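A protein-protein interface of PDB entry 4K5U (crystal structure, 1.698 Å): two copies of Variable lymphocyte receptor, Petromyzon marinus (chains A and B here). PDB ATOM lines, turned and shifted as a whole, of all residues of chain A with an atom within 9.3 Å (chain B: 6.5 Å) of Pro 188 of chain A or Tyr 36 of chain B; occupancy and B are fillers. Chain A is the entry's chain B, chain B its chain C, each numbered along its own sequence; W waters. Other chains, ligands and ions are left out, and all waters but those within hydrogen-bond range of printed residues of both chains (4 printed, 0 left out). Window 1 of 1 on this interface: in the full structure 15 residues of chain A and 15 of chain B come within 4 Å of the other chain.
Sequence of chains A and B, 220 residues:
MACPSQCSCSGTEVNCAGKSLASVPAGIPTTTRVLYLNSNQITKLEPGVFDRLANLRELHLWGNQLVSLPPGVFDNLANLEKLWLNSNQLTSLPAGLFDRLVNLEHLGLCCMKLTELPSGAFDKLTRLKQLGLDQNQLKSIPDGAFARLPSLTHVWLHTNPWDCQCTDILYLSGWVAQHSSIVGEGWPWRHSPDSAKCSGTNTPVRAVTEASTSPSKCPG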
ATOM      1  N   LYS A  82     -10.450  32.801   7.872  1.00  0.00           N
ATOM      2  CA  LYS A  82     -10.205  32.491   6.433  1.00  0.00           C
ATOM      3  C   LYS A  82     -10.559  33.719   5.605  1.00  0.00           C
ATOM      4  O   LYS A  82     -11.643  34.346   5.798  1.00  0.00           O
ATOM      5  CB  LYS A  82     -11.126  31.344   5.974  1.00  0.00           C
ATOM      6  CG  LYS A  82     -10.941  30.034   6.777  1.00  0.00           C
ATOM      7  CD  LYS A  82     -11.841  28.883   6.312  1.00  0.00           C
ATOM      8  CE  LYS A  82     -11.460  27.595   6.991  1.00  0.00           C
ATOM      9  NZ  LYS A  82     -12.365  26.532   6.550  1.00  0.00           N
ATOM     10  N   TRP A  84     -10.570  35.060   1.556  1.00  0.00           N
ATOM     11  CA  TRP A  84     -10.398  34.545   0.179  1.00  0.00           C
ATOM     12  C   TRP A  84     -10.561  35.684  -0.787  1.00  0.00           C
ATOM     13  O   TRP A  84     -11.661  36.222  -0.943  1.00  0.00           O
ATOM     14  CB  TRP A  84     -11.491  33.492  -0.159  1.00  0.00           C
ATOM     15  CG  TRP A  84     -11.560  32.298   0.687  1.00  0.00           C
ATOM     16  CD1 TRP A  84     -12.534  32.009   1.663  1.00  0.00           C
ATOM     17  CD2 TRP A  84     -10.591  31.260   0.792  1.00  0.00           C
ATOM     18  NE1 TRP A  84     -12.222  30.803   2.294  1.00  0.00           N
ATOM     19  CE2 TRP A  84     -11.021  30.368   1.810  1.00  0.00           C
ATOM     20  CE3 TRP A  84      -9.357  31.026   0.151  1.00  0.00           C
ATOM     21  CZ2 TRP A  84     -10.301  29.194   2.157  1.00  0.00           C
ATOM     22  CZ3 TRP A  84      -8.631  29.844   0.507  1.00  0.00           C
ATOM     23  CH2 TRP A  84      -9.111  28.974   1.508  1.00  0.00           C
ATOM     24  N   HIS A 106      -6.197  30.632   6.878  1.00  0.00           N
ATOM     25  CA  HIS A 106      -6.181  30.366   5.396  1.00  0.00           C
ATOM     26  C   HIS A 106      -6.195  31.739   4.712  1.00  0.00           C
ATOM     27  O   HIS A 106      -7.061  32.576   4.977  1.00  0.00           O
ATOM     28  CB  HIS A 106      -7.458  29.639   5.038  1.00  0.00           C
ATOM     29  CG  HIS A 106      -7.530  28.276   5.633  1.00  0.00           C
ATOM     30  ND1 HIS A 106      -7.269  27.132   4.903  1.00  0.00           N
ATOM     31  CD2 HIS A 106      -7.793  27.875   6.902  1.00  0.00           C
ATOM     32  CE1 HIS A 106      -7.382  26.075   5.702  1.00  0.00           C
ATOM     33  NE2 HIS A 106      -7.698  26.500   6.917  1.00  0.00           N
ATOM     34  N   GLN A 130      -2.389  27.935   5.529  1.00  0.00           N
ATOM     35  CA  GLN A 130      -2.457  27.735   4.043  1.00  0.00           C
ATOM     36  C   GLN A 130      -2.381  29.106   3.367  1.00  0.00           C
ATOM     37  O   GLN A 130      -3.142  30.030   3.687  1.00  0.00           O
ATOM     38  CB  GLN A 130      -3.784  26.924   3.690  1.00  0.00           C
ATOM     39  CG  GLN A 130      -3.806  25.551   4.437  1.00  0.00           C
ATOM     40  CD  GLN A 130      -4.695  24.456   3.823  1.00  0.00           C
ATOM     41  OE1 GLN A 130      -5.090  24.535   2.663  1.00  0.00           O
ATOM     42  NE2 GLN A 130      -4.971  23.421   4.595  1.00  0.00           N
ATOM     43  N   HIS A 154       0.974  24.598   4.033  1.00  0.00           N
ATOM     44  CA  HIS A 154       0.523  24.388   2.622  1.00  0.00           C
ATOM     45  C   HIS A 154       0.732  25.697   1.935  1.00  0.00           C
ATOM     46  O   HIS A 154       0.192  26.717   2.344  1.00  0.00           O
ATOM     47  CB  HIS A 154      -1.000  24.002   2.545  1.00  0.00           C
ATOM     48  CG  HIS A 154      -1.347  22.732   3.219  1.00  0.00           C
ATOM     49  ND1 HIS A 154      -1.625  22.662   4.594  1.00  0.00           N
ATOM     50  CD2 HIS A 154      -1.400  21.458   2.742  1.00  0.00           C
ATOM     51  CE1 HIS A 154      -1.808  21.380   4.905  1.00  0.00           C
ATOM     52  NE2 HIS A 154      -1.814  20.654   3.769  1.00  0.00           N
ATOM     53  N   TRP A 156       1.021  27.471  -2.156  1.00  0.00           N
ATOM     54  CA  TRP A 156       0.956  27.253  -3.646  1.00  0.00           C
ATOM     55  C   TRP A 156       1.744  28.415  -4.240  1.00  0.00           C
ATOM     56  O   TRP A 156       1.550  29.597  -3.946  1.00  0.00           O
ATOM     57  CB  TRP A 156      -0.505  27.431  -4.046  1.00  0.00           C
ATOM     58  CG  TRP A 156      -1.490  26.365  -3.693  1.00  0.00           C
ATOM     59  CD1 TRP A 156      -2.087  25.469  -4.580  1.00  0.00           C
ATOM     60  CD2 TRP A 156      -2.093  26.106  -2.419  1.00  0.00           C
ATOM     61  NE1 TRP A 156      -2.978  24.680  -3.951  1.00  0.00           N
ATOM     62  CE2 TRP A 156      -3.003  25.023  -2.599  1.00  0.00           C
ATOM     63  CE3 TRP A 156      -1.923  26.688  -1.118  1.00  0.00           C
ATOM     64  CZ2 TRP A 156      -3.813  24.547  -1.572  1.00  0.00           C
ATOM     65  CZ3 TRP A 156      -2.716  26.177  -0.054  1.00  0.00           C
ATOM     66  CH2 TRP A 156      -3.638  25.103  -0.301  1.00  0.00           C
ATOM     67  N   GLY A 184       2.843  22.944  -3.171  1.00  0.00           N
ATOM     68  CA  GLY A 184       1.934  22.080  -3.913  1.00  0.00           C
ATOM     69  C   GLY A 184       0.989  22.787  -4.853  1.00  0.00           C
ATOM     70  O   GLY A 184       1.157  23.943  -5.174  1.00  0.00           O
ATOM     71  N   GLU A 185       0.010  22.004  -5.291  1.00  0.00           N
ATOM     72  CA  GLU A 185      -0.957  22.506  -6.259  1.00  0.00           C
ATOM     73  C   GLU A 185      -2.293  21.843  -6.092  1.00  0.00           C
ATOM     74  O   GLU A 185      -2.416  20.794  -5.512  1.00  0.00           O
ATOM     75  CB  GLU A 185      -0.438  22.259  -7.688  1.00  0.00           C
ATOM     76  CG  GLU A 185      -0.346  20.893  -8.113  1.00  0.00           C
ATOM     77  CD  GLU A 185       0.273  20.839  -9.541  1.00  0.00           C
ATOM     78  OE1 GLU A 185       1.499  20.689  -9.692  1.00  0.00           O
ATOM     79  OE2 GLU A 185      -0.457  21.075 -10.517  1.00  0.00           O
ATOM     80  N   GLY A 186      -3.325  22.467  -6.651  1.00  0.00           N
ATOM     81  CA  GLY A 186      -4.621  21.855  -6.668  1.00  0.00           C
ATOM     82  C   GLY A 186      -5.470  22.217  -5.471  1.00  0.00           C
ATOM     83  O   GLY A 186      -4.987  22.893  -4.542  1.00  0.00           O
ATOM     84  N   TRP A 187      -6.777  21.892  -5.592  1.00  0.00           N
ATOM     85  CA  TRP A 187      -7.676  22.079  -4.493  1.00  0.00           C
ATOM     86  C   TRP A 187      -8.499  20.845  -4.266  1.00  0.00           C
ATOM     87  O   TRP A 187      -9.253  20.392  -5.166  1.00  0.00           O
ATOM     88  CB  TRP A 187      -8.605  23.286  -4.751  1.00  0.00           C
ATOM     89  CG  TRP A 187      -9.423  23.598  -3.585  1.00  0.00           C
ATOM     90  CD1 TRP A 187     -10.783  23.470  -3.483  1.00  0.00           C
ATOM     91  CD2 TRP A 187      -8.953  24.070  -2.279  1.00  0.00           C
ATOM     92  NE1 TRP A 187     -11.190  23.860  -2.206  1.00  0.00           N
ATOM     93  CE2 TRP A 187     -10.087  24.197  -1.452  1.00  0.00           C
ATOM     94  CE3 TRP A 187      -7.689  24.387  -1.756  1.00  0.00           C
ATOM     95  CZ2 TRP A 187     -10.001  24.642  -0.104  1.00  0.00           C
ATOM     96  CZ3 TRP A 187      -7.596  24.829  -0.417  1.00  0.00           C
ATOM     97  CH2 TRP A 187      -8.748  24.937   0.394  1.00  0.00           C
ATOM     98  N   PRO A 188      -8.387  20.210  -3.066  1.00  0.00           N
ATOM     99  CA  PRO A 188      -7.446  20.556  -1.988  1.00  0.00           C
ATOM    100  C   PRO A 188      -6.029  20.310  -2.383  1.00  0.00           C
ATOM    101  O   PRO A 188      -5.752  19.740  -3.428  1.00  0.00           O
ATOM    102  CB  PRO A 188      -7.801  19.609  -0.836  1.00  0.00           C
ATOM    103  CG  PRO A 188      -9.023  18.668  -1.370  1.00  0.00           C
ATOM    104  CD  PRO A 188      -9.194  18.997  -2.845  1.00  0.00           C
ATOM    105  N   TRP A 189      -5.108  20.719  -1.502  1.00  0.00           N
ATOM    106  CA  TRP A 189      -3.663  20.702  -1.883  1.00  0.00           C
ATOM    107  C   TRP A 189      -3.153  19.330  -2.150  1.00  0.00           C
ATOM    108  O   TRP A 189      -3.477  18.345  -1.449  1.00  0.00           O
ATOM    109  CB  TRP A 189      -2.902  21.289  -0.652  1.00  0.00           C
ATOM    110  CG  TRP A 189      -1.385  21.395  -0.754  1.00  0.00           C
ATOM    111  CD1 TRP A 189      -0.695  22.503  -1.014  1.00  0.00           C
ATOM    112  CD2 TRP A 189      -0.471  20.408  -0.335  1.00  0.00           C
ATOM    113  NE1 TRP A 189       0.687  22.246  -0.901  1.00  0.00           N
ATOM    114  CE2 TRP A 189       0.834  20.977  -0.426  1.00  0.00           C
ATOM    115  CE3 TRP A 189      -0.624  19.089   0.110  1.00  0.00           C
ATOM    116  CZ2 TRP A 189       2.037  20.215  -0.072  1.00  0.00           C
ATOM    117  CZ3 TRP A 189       0.500  18.357   0.457  1.00  0.00           C
ATOM    118  CH2 TRP A 189       1.827  18.897   0.324  1.00  0.00           C
ATOM    119  N   ARG A 190      -2.306  19.220  -3.196  1.00  0.00           N
ATOM    120  CA  ARG A 190      -1.522  17.966  -3.493  1.00  0.00           C
ATOM    121  C   ARG A 190      -0.056  18.346  -3.560  1.00  0.00           C
ATOM    122  O   ARG A 190       0.259  19.411  -4.045  1.00  0.00           O
ATOM    123  CB  ARG A 190      -1.947  17.286  -4.837  1.00  0.00           C
ATOM    124  CG  ARG A 190      -3.458  17.022  -4.854  1.00  0.00           C
ATOM    125  CD  ARG A 190      -4.041  16.587  -6.227  1.00  0.00           C
ATOM    126  NE  ARG A 190      -3.110  16.868  -7.297  1.00  0.00           N
ATOM    127  CZ  ARG A 190      -3.272  17.762  -8.267  1.00  0.00           C
ATOM    128  NH1 ARG A 190      -4.364  18.524  -8.332  1.00  0.00           N
ATOM    129  NH2 ARG A 190      -2.294  17.907  -9.167  1.00  0.00           N
ATOM    130  N   HIS A 191       0.832  17.447  -3.143  1.00  0.00           N
ATOM    131  CA  HIS A 191       2.227  17.735  -3.040  1.00  0.00           C
ATOM    132  C   HIS A 191       2.857  17.929  -4.421  1.00  0.00           C
ATOM    133  O   HIS A 191       2.602  17.089  -5.287  1.00  0.00           O
ATOM    134  CB  HIS A 191       2.972  16.611  -2.316  1.00  0.00           C
ATOM    135  CG  HIS A 191       4.400  16.960  -2.029  1.00  0.00           C
ATOM    136  ND1 HIS A 191       5.446  16.055  -2.171  1.00  0.00           N
ATOM    137  CD2 HIS A 191       4.967  18.139  -1.643  1.00  0.00           C
ATOM    138  CE1 HIS A 191       6.577  16.649  -1.805  1.00  0.00           C
ATOM    139  NE2 HIS A 191       6.311  17.911  -1.512  1.00  0.00           N
ATOM    140  N   CYS B   7      -1.897   9.239  -1.238  1.00  0.00           N
ATOM    141  CA  CYS B   7      -2.435  10.488  -0.736  1.00  0.00           C
ATOM    142  C   CYS B   7      -1.337  11.550  -0.620  1.00  0.00           C
ATOM    143  O   CYS B   7      -0.157  11.233  -0.761  1.00  0.00           O
ATOM    144  CB  CYS B   7      -3.010  10.183   0.627  1.00  0.00           C
ATOM    145  SG  CYS B   7      -4.339   8.874   0.454  1.00  0.00           S
ATOM    146  N   GLU B  13      -3.666  17.793   7.448  1.00  0.00           N
ATOM    147  CA  GLU B  13      -4.671  17.536   6.412  1.00  0.00           C
ATOM    148  C   GLU B  13      -4.189  16.342   5.568  1.00  0.00           C
ATOM    149  O   GLU B  13      -2.977  16.250   5.219  1.00  0.00           O
ATOM    150  CB  GLU B  13      -4.734  18.782   5.544  1.00  0.00           C
ATOM    151  CG  GLU B  13      -5.685  18.614   4.262  1.00  0.00           C
ATOM    152  CD  GLU B  13      -5.948  19.958   3.570  1.00  0.00           C
ATOM    153  OE1 GLU B  13      -6.448  20.917   4.262  1.00  0.00           O
ATOM    154  OE2 GLU B  13      -5.695  20.099   2.331  1.00  0.00           O
ATOM    155  N   VAL B  14      -5.087  15.465   5.260  1.00  0.00           N
ATOM    156  CA  VAL B  14      -4.735  14.271   4.398  1.00  0.00           C
ATOM    157  C   VAL B  14      -5.677  14.313   3.203  1.00  0.00           C
ATOM    158  O   VAL B  14      -6.902  14.278   3.364  1.00  0.00           O
ATOM    159  CB  VAL B  14      -4.891  13.005   5.237  1.00  0.00           C
ATOM    160  CG1 VAL B  14      -4.684  11.802   4.410  1.00  0.00           C
ATOM    161  CG2 VAL B  14      -3.812  13.031   6.277  1.00  0.00           C
ATOM    162  N   ASN B  15      -5.067  14.326   2.005  1.00  0.00           N
ATOM    163  CA  ASN B  15      -5.897  14.397   0.743  1.00  0.00           C
ATOM    164  C   ASN B  15      -5.740  13.080   0.000  1.00  0.00           C
ATOM    165  O   ASN B  15      -4.693  12.831  -0.656  1.00  0.00           O
ATOM    166  CB  ASN B  15      -5.395  15.529  -0.119  1.00  0.00           C
ATOM    167  CG  ASN B  15      -6.190  15.652  -1.400  1.00  0.00           C
ATOM    168  OD1 ASN B  15      -7.148  14.858  -1.614  1.00  0.00           O
ATOM    169  ND2 ASN B  15      -5.851  16.605  -2.218  1.00  0.00           N
ATOM    170  N   CYS B  16      -6.809  12.294   0.071  1.00  0.00           N
ATOM    171  CA  CYS B  16      -6.862  11.024  -0.650  1.00  0.00           C
ATOM    172  C   CYS B  16      -7.970  11.104  -1.675  1.00  0.00           C
ATOM    173  O   CYS B  16      -8.499  10.006  -1.978  1.00  0.00           O
ATOM    174  CB  CYS B  16      -7.185   9.867   0.328  1.00  0.00           C
ATOM    175  SG  CYS B  16      -5.990   9.501   1.598  1.00  0.00           S
ATOM    176  N   ALA B  17      -8.364  12.304  -2.121  1.00  0.00           N
ATOM    177  CA  ALA B  17      -9.564  12.453  -3.003  1.00  0.00           C
ATOM    178  C   ALA B  17      -9.229  11.995  -4.425  1.00  0.00           C
ATOM    179  O   ALA B  17      -8.164  12.312  -4.963  1.00  0.00           O
ATOM    180  CB  ALA B  17     -10.009  13.875  -3.049  1.00  0.00           C
ATOM    181  N   GLY B  18     -10.164  11.292  -5.036  1.00  0.00           N
ATOM    182  CA  GLY B  18     -10.070  11.100  -6.524  1.00  0.00           C
ATOM    183  C   GLY B  18      -8.973  10.134  -6.905  1.00  0.00           C
ATOM    184  O   GLY B  18      -8.353  10.269  -8.021  1.00  0.00           O
ATOM    185  N   VAL B  34      -8.180  16.951   9.094  1.00  0.00           N
ATOM    186  CA  VAL B  34      -9.081  17.161   7.920  1.00  0.00           C
ATOM    187  C   VAL B  34      -8.778  16.016   6.941  1.00  0.00           C
ATOM    188  O   VAL B  34      -7.623  15.835   6.561  1.00  0.00           O
ATOM    189  CB  VAL B  34      -8.798  18.513   7.322  1.00  0.00           C
ATOM    190  CG1 VAL B  34      -9.641  18.636   6.012  1.00  0.00           C
ATOM    191  CG2 VAL B  34      -9.374  19.594   8.216  1.00  0.00           C
ATOM    192  N   LEU B  35      -9.757  15.203   6.600  1.00  0.00           N
ATOM    193  CA  LEU B  35      -9.485  14.044   5.830  1.00  0.00           C
ATOM    194  C   LEU B  35     -10.372  14.074   4.552  1.00  0.00           C
ATOM    195  O   LEU B  35     -11.612  14.111   4.670  1.00  0.00           O
ATOM    196  CB  LEU B  35      -9.666  12.770   6.682  1.00  0.00           C
ATOM    197  CG  LEU B  35      -9.586  11.466   5.879  1.00  0.00           C
ATOM    198  CD1 LEU B  35      -8.183  11.273   5.199  1.00  0.00           C
ATOM    199  CD2 LEU B  35      -9.737  10.260   6.910  1.00  0.00           C
ATOM    200  N   TYR B  36      -9.760  14.098   3.375  1.00  0.00           N
ATOM    201  CA  TYR B  36     -10.561  14.051   2.170  1.00  0.00           C
ATOM    202  C   TYR B  36     -10.543  12.652   1.598  1.00  0.00           C
ATOM    203  O   TYR B  36      -9.466  12.179   1.115  1.00  0.00           O
ATOM    204  CB  TYR B  36      -9.970  15.015   1.118  1.00  0.00           C
ATOM    205  CG  TYR B  36     -10.055  16.487   1.504  1.00  0.00           C
ATOM    206  CD1 TYR B  36     -11.228  17.213   1.336  1.00  0.00           C
ATOM    207  CD2 TYR B  36      -8.958  17.164   2.054  1.00  0.00           C
ATOM    208  CE1 TYR B  36     -11.269  18.614   1.653  1.00  0.00           C
ATOM    209  CE2 TYR B  36      -8.998  18.572   2.377  1.00  0.00           C
ATOM    210  CZ  TYR B  36     -10.198  19.260   2.184  1.00  0.00           C
ATOM    211  OH  TYR B  36     -10.401  20.618   2.427  1.00  0.00           O
ATOM    212  N   LEU B  37     -11.679  11.949   1.600  1.00  0.00           N
ATOM    213  CA  LEU B  37     -11.767  10.644   0.972  1.00  0.00           C
ATOM    214  C   LEU B  37     -12.848  10.717  -0.104  1.00  0.00           C
ATOM    215  O   LEU B  37     -13.305   9.619  -0.575  1.00  0.00           O
ATOM    216  CB  LEU B  37     -12.115   9.561   1.973  1.00  0.00           C
ATOM    217  CG  LEU B  37     -10.929   9.269   2.865  1.00  0.00           C
ATOM    218  CD1 LEU B  37     -11.468   8.662   4.136  1.00  0.00           C
ATOM    219  CD2 LEU B  37     -10.035   8.242   2.144  1.00  0.00           C
ATOM    220  N   ASN B  38     -13.241  11.896  -0.494  1.00  0.00           N
ATOM    221  CA  ASN B  38     -14.346  12.035  -1.473  1.00  0.00           C
ATOM    222  C   ASN B  38     -13.943  11.523  -2.864  1.00  0.00           C
ATOM    223  O   ASN B  38     -12.757  11.472  -3.181  1.00  0.00           O
ATOM    224  CB  ASN B  38     -14.750  13.504  -1.609  1.00  0.00           C
ATOM    225  CG  ASN B  38     -13.574  14.427  -1.959  1.00  0.00           C
ATOM    226  OD1 ASN B  38     -12.781  14.819  -1.069  1.00  0.00           O
ATOM    227  ND2 ASN B  38     -13.468  14.809  -3.243  1.00  0.00           N
ATOM    228  N   ASN B  40     -13.970   8.826  -4.684  1.00  0.00           N
ATOM    229  CA  ASN B  40     -13.273   7.560  -4.845  1.00  0.00           C
ATOM    230  C   ASN B  40     -14.300   6.485  -5.270  1.00  0.00           C
ATOM    231  O   ASN B  40     -15.358   6.863  -5.733  1.00  0.00           O
ATOM    232  CB  ASN B  40     -12.508   7.158  -3.577  1.00  0.00           C
ATOM    233  CG  ASN B  40     -11.180   7.905  -3.460  1.00  0.00           C
ATOM    234  OD1 ASN B  40     -10.287   7.701  -4.277  1.00  0.00           O
ATOM    235  ND2 ASN B  40     -11.021   8.720  -2.410  1.00  0.00           N
ATOM    236  N   GLU B  58     -12.917  17.387  10.297  1.00  0.00           N
ATOM    237  CA  GLU B  58     -13.703  17.393   9.007  1.00  0.00           C
ATOM    238  C   GLU B  58     -13.481  16.110   8.293  1.00  0.00           C
ATOM    239  O   GLU B  58     -12.345  15.667   8.128  1.00  0.00           O
ATOM    240  CB  GLU B  58     -13.344  18.574   8.123  1.00  0.00           C
ATOM    241  CG  GLU B  58     -13.444  19.951   8.796  1.00  0.00           C
ATOM    242  CD  GLU B  58     -13.078  21.075   7.791  1.00  0.00           C
ATOM    243  OE1 GLU B  58     -13.167  20.873   6.536  1.00  0.00           O
ATOM    244  OE2 GLU B  58     -12.689  22.124   8.299  1.00  0.00           O
ATOM    245  N   LEU B  59     -14.560  15.485   7.823  1.00  0.00           N
ATOM    246  CA  LEU B  59     -14.441  14.141   7.206  1.00  0.00           C
ATOM    247  C   LEU B  59     -15.300  14.193   5.896  1.00  0.00           C
ATOM    248  O   LEU B  59     -16.527  14.382   5.967  1.00  0.00           O
ATOM    249  CB  LEU B  59     -14.905  13.085   8.161  1.00  0.00           C
ATOM    250  CG  LEU B  59     -14.968  11.620   7.604  1.00  0.00           C
ATOM    251  CD1 LEU B  59     -13.604  11.195   6.999  1.00  0.00           C
ATOM    252  CD2 LEU B  59     -15.435  10.577   8.637  1.00  0.00           C
ATOM    253  N   HIS B  60     -14.581  14.125   4.777  1.00  0.00           N
ATOM    254  CA  HIS B  60     -15.251  14.278   3.465  1.00  0.00           C
ATOM    255  C   HIS B  60     -15.378  12.871   2.874  1.00  0.00           C
ATOM    256  O   HIS B  60     -14.346  12.250   2.474  1.00  0.00           O
ATOM    257  CB  HIS B  60     -14.398  15.164   2.538  1.00  0.00           C
ATOM    258  CG  HIS B  60     -14.377  16.614   2.888  1.00  0.00           C
ATOM    259  ND1 HIS B  60     -13.779  17.096   4.042  1.00  0.00           N
ATOM    260  CD2 HIS B  60     -14.895  17.708   2.253  1.00  0.00           C
ATOM    261  CE1 HIS B  60     -13.904  18.411   4.093  1.00  0.00           C
ATOM    262  NE2 HIS B  60     -14.600  18.799   3.040  1.00  0.00           N
ATOM    263  N   LEU B  61     -16.609  12.354   2.761  1.00  0.00           N
ATOM    264  CA  LEU B  61     -16.835  11.046   2.213  1.00  0.00           C
ATOM    265  C   LEU B  61     -17.743  11.144   1.005  1.00  0.00           C
ATOM    266  O   LEU B  61     -18.194  10.082   0.533  1.00  0.00           O
ATOM    267  CB  LEU B  61     -17.408  10.130   3.264  1.00  0.00           C
ATOM    268  CG  LEU B  61     -16.372   9.703   4.338  1.00  0.00           C
ATOM    269  CD1 LEU B  61     -17.176   8.981   5.441  1.00  0.00           C
ATOM    270  CD2 LEU B  61     -15.378   8.747   3.573  1.00  0.00           C
ATOM    271  N   TRP B  62     -18.006  12.343   0.550  1.00  0.00           N
ATOM    272  CA  TRP B  62     -19.027  12.553  -0.497  1.00  0.00           C
ATOM    273  C   TRP B  62     -18.531  11.976  -1.812  1.00  0.00           C
ATOM    274  O   TRP B  62     -17.313  11.821  -2.036  1.00  0.00           O
ATOM    275  CB  TRP B  62     -19.324  14.079  -0.644  1.00  0.00           C
ATOM    276  CG  TRP B  62     -18.177  14.995  -0.870  1.00  0.00           C
ATOM    277  CD1 TRP B  62     -17.394  15.600   0.112  1.00  0.00           C
ATOM    278  CD2 TRP B  62     -17.625  15.428  -2.121  1.00  0.00           C
ATOM    279  NE1 TRP B  62     -16.431  16.360  -0.452  1.00  0.00           N
ATOM    280  CE2 TRP B  62     -16.530  16.265  -1.824  1.00  0.00           C
ATOM    281  CE3 TRP B  62     -17.945  15.152  -3.478  1.00  0.00           C
ATOM    282  CZ2 TRP B  62     -15.759  16.901  -2.814  1.00  0.00           C
ATOM    283  CZ3 TRP B  62     -17.172  15.786  -4.484  1.00  0.00           C
ATOM    284  CH2 TRP B  62     -16.103  16.671  -4.136  1.00  0.00           C
HETATM  285  O   HOH W   1      -5.861  22.218   0.918  1.00  0.00           O
HETATM  286  O   HOH W   2      -6.814  21.453   6.744  1.00  0.00           O
HETATM  287  O   HOH W   3      -2.248  17.957   2.991  1.00  0.00           O
HETATM  288  O   HOH W   4      -4.249  18.302   1.169  1.00  0.00           O
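Among the printed residues, pairs that only touch across the chains: His 154 of chain A with Glu 13 of chain B (3.9 Å), Pro 188 of chain A with Glu 13 of chain B (3.8 Å), Pro 188 of chain A with Tyr 36 of chain B (3.6 Å), Trp 189 of chain A with Glu 13 of chain B (3.9 Å) and Arg 190 of chain A with Asn 15 of chain B (3.6 Å).
The backbone carbonyl oxygen (O) of Trp 189 of chain A lies within hydrogen-bond range of the side-chain amide nitrogen (ND2) of Asn 15 of chain B (3.0 Å). The backbone carbonyl oxygen of Pro 188 of chain A sits at hydrogen-bond distance from the side-chain amide nitrogen of Asn 15 of chain B, 3.4 Å away. OE1 of Glu 13 of chain B is in hydrogen-bond range of NE2 of Gln 130 of chain A (2.9 Å).
The side-chain amide nitrogen (NE2) of Gln 130 of chain A is in hydrogen-bond range of a ring nitrogen (ND1) of His 154 of chain A. The side-chain amide oxygen (OD1) of Asn 15 of chain B sits at hydrogen-bond distance from the backbone NH (N) of Ala 17 of chain B (2.9 Å). The backbone NH of Cys 16 of chain B is in hydrogen-bond range of the backbone carbonyl oxygen of Tyr 36 of chain B, at 2.9 Å. The side-chain sulfur of Cys 7 of chain B is disulfide-bonded to the side-chain sulfur of Cys 16 of chain B (2.1 Å). The side-chain carboxylate (OE2) of Glu 185 of chain A is in salt-bridge range of the guanidinium group (NH2) of Arg 190 of chain A. N of Ala 17 of chain B sits at hydrogen-bond distance from O of Tyr 36 of chain B.
Of chain B, only Glu 13 (3.8 Å), Asn 15 (3.4 Å) and Tyr 36 (3.6 Å) come within 4 Å of Pro 188 of chain A. Tyr 36 of chain B touches one residue of chain A. No residue of chain A comes within 4 Å of Leu 35 of chain B. Printed residues of chain B within 4 Å of His 154 of chain A: Glu 13. Printed residues of chain B within 4 Å of Trp 189 of chain A: Glu 13 and Asn 15. Printed residues of chain B within 4 Å of Arg 190 of chain A: Asn 15 (3.6 Å). Printed residues of chain B within 4 Å of Gln 130 of chain A: Glu 13 (2.9 Å). Of the printed residues of chain A, Glu 13 of chain B touches Gln 130, His 154, Pro 188 and Trp 189. Asn 40 of chain B touches none of the printed residues of chain A.
Of the 14 printed residues of chain A, 5 touch a printed residue of chain B. Along chain B the printed residues that touch a printed residue of chain A span positions 13 to 36. Among the printed residues, 8 pairs touch across the chains. Among the printed residues, no Asp or Glu carboxylate lies within 4 Å of a Lys or Arg side-chain nitrogen of the other chain.
Water W1 lies within hydrogen-bond range of OE2 of Glu 13 of chain B, N of Trp 189 of chain A and OE1 of Gln 130 of chain A. Water W2 bridges OE1 of Glu 13 of chain B (2.6 Å) and NE2 of Gln 130 of chain A (3.4 Å). Water W4 lies within hydrogen-bond range of OE2 of Glu 13 of chain B and O of Trp 189 of chain A. Water W3 lies within hydrogen-bond range of a ring nitrogen (NE2) of His 154 of chain A (2.8 Å) and the backbone carbonyl oxygen (O) of Glu 13 of chain B (2.9 Å).
No position is printed for both chains.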
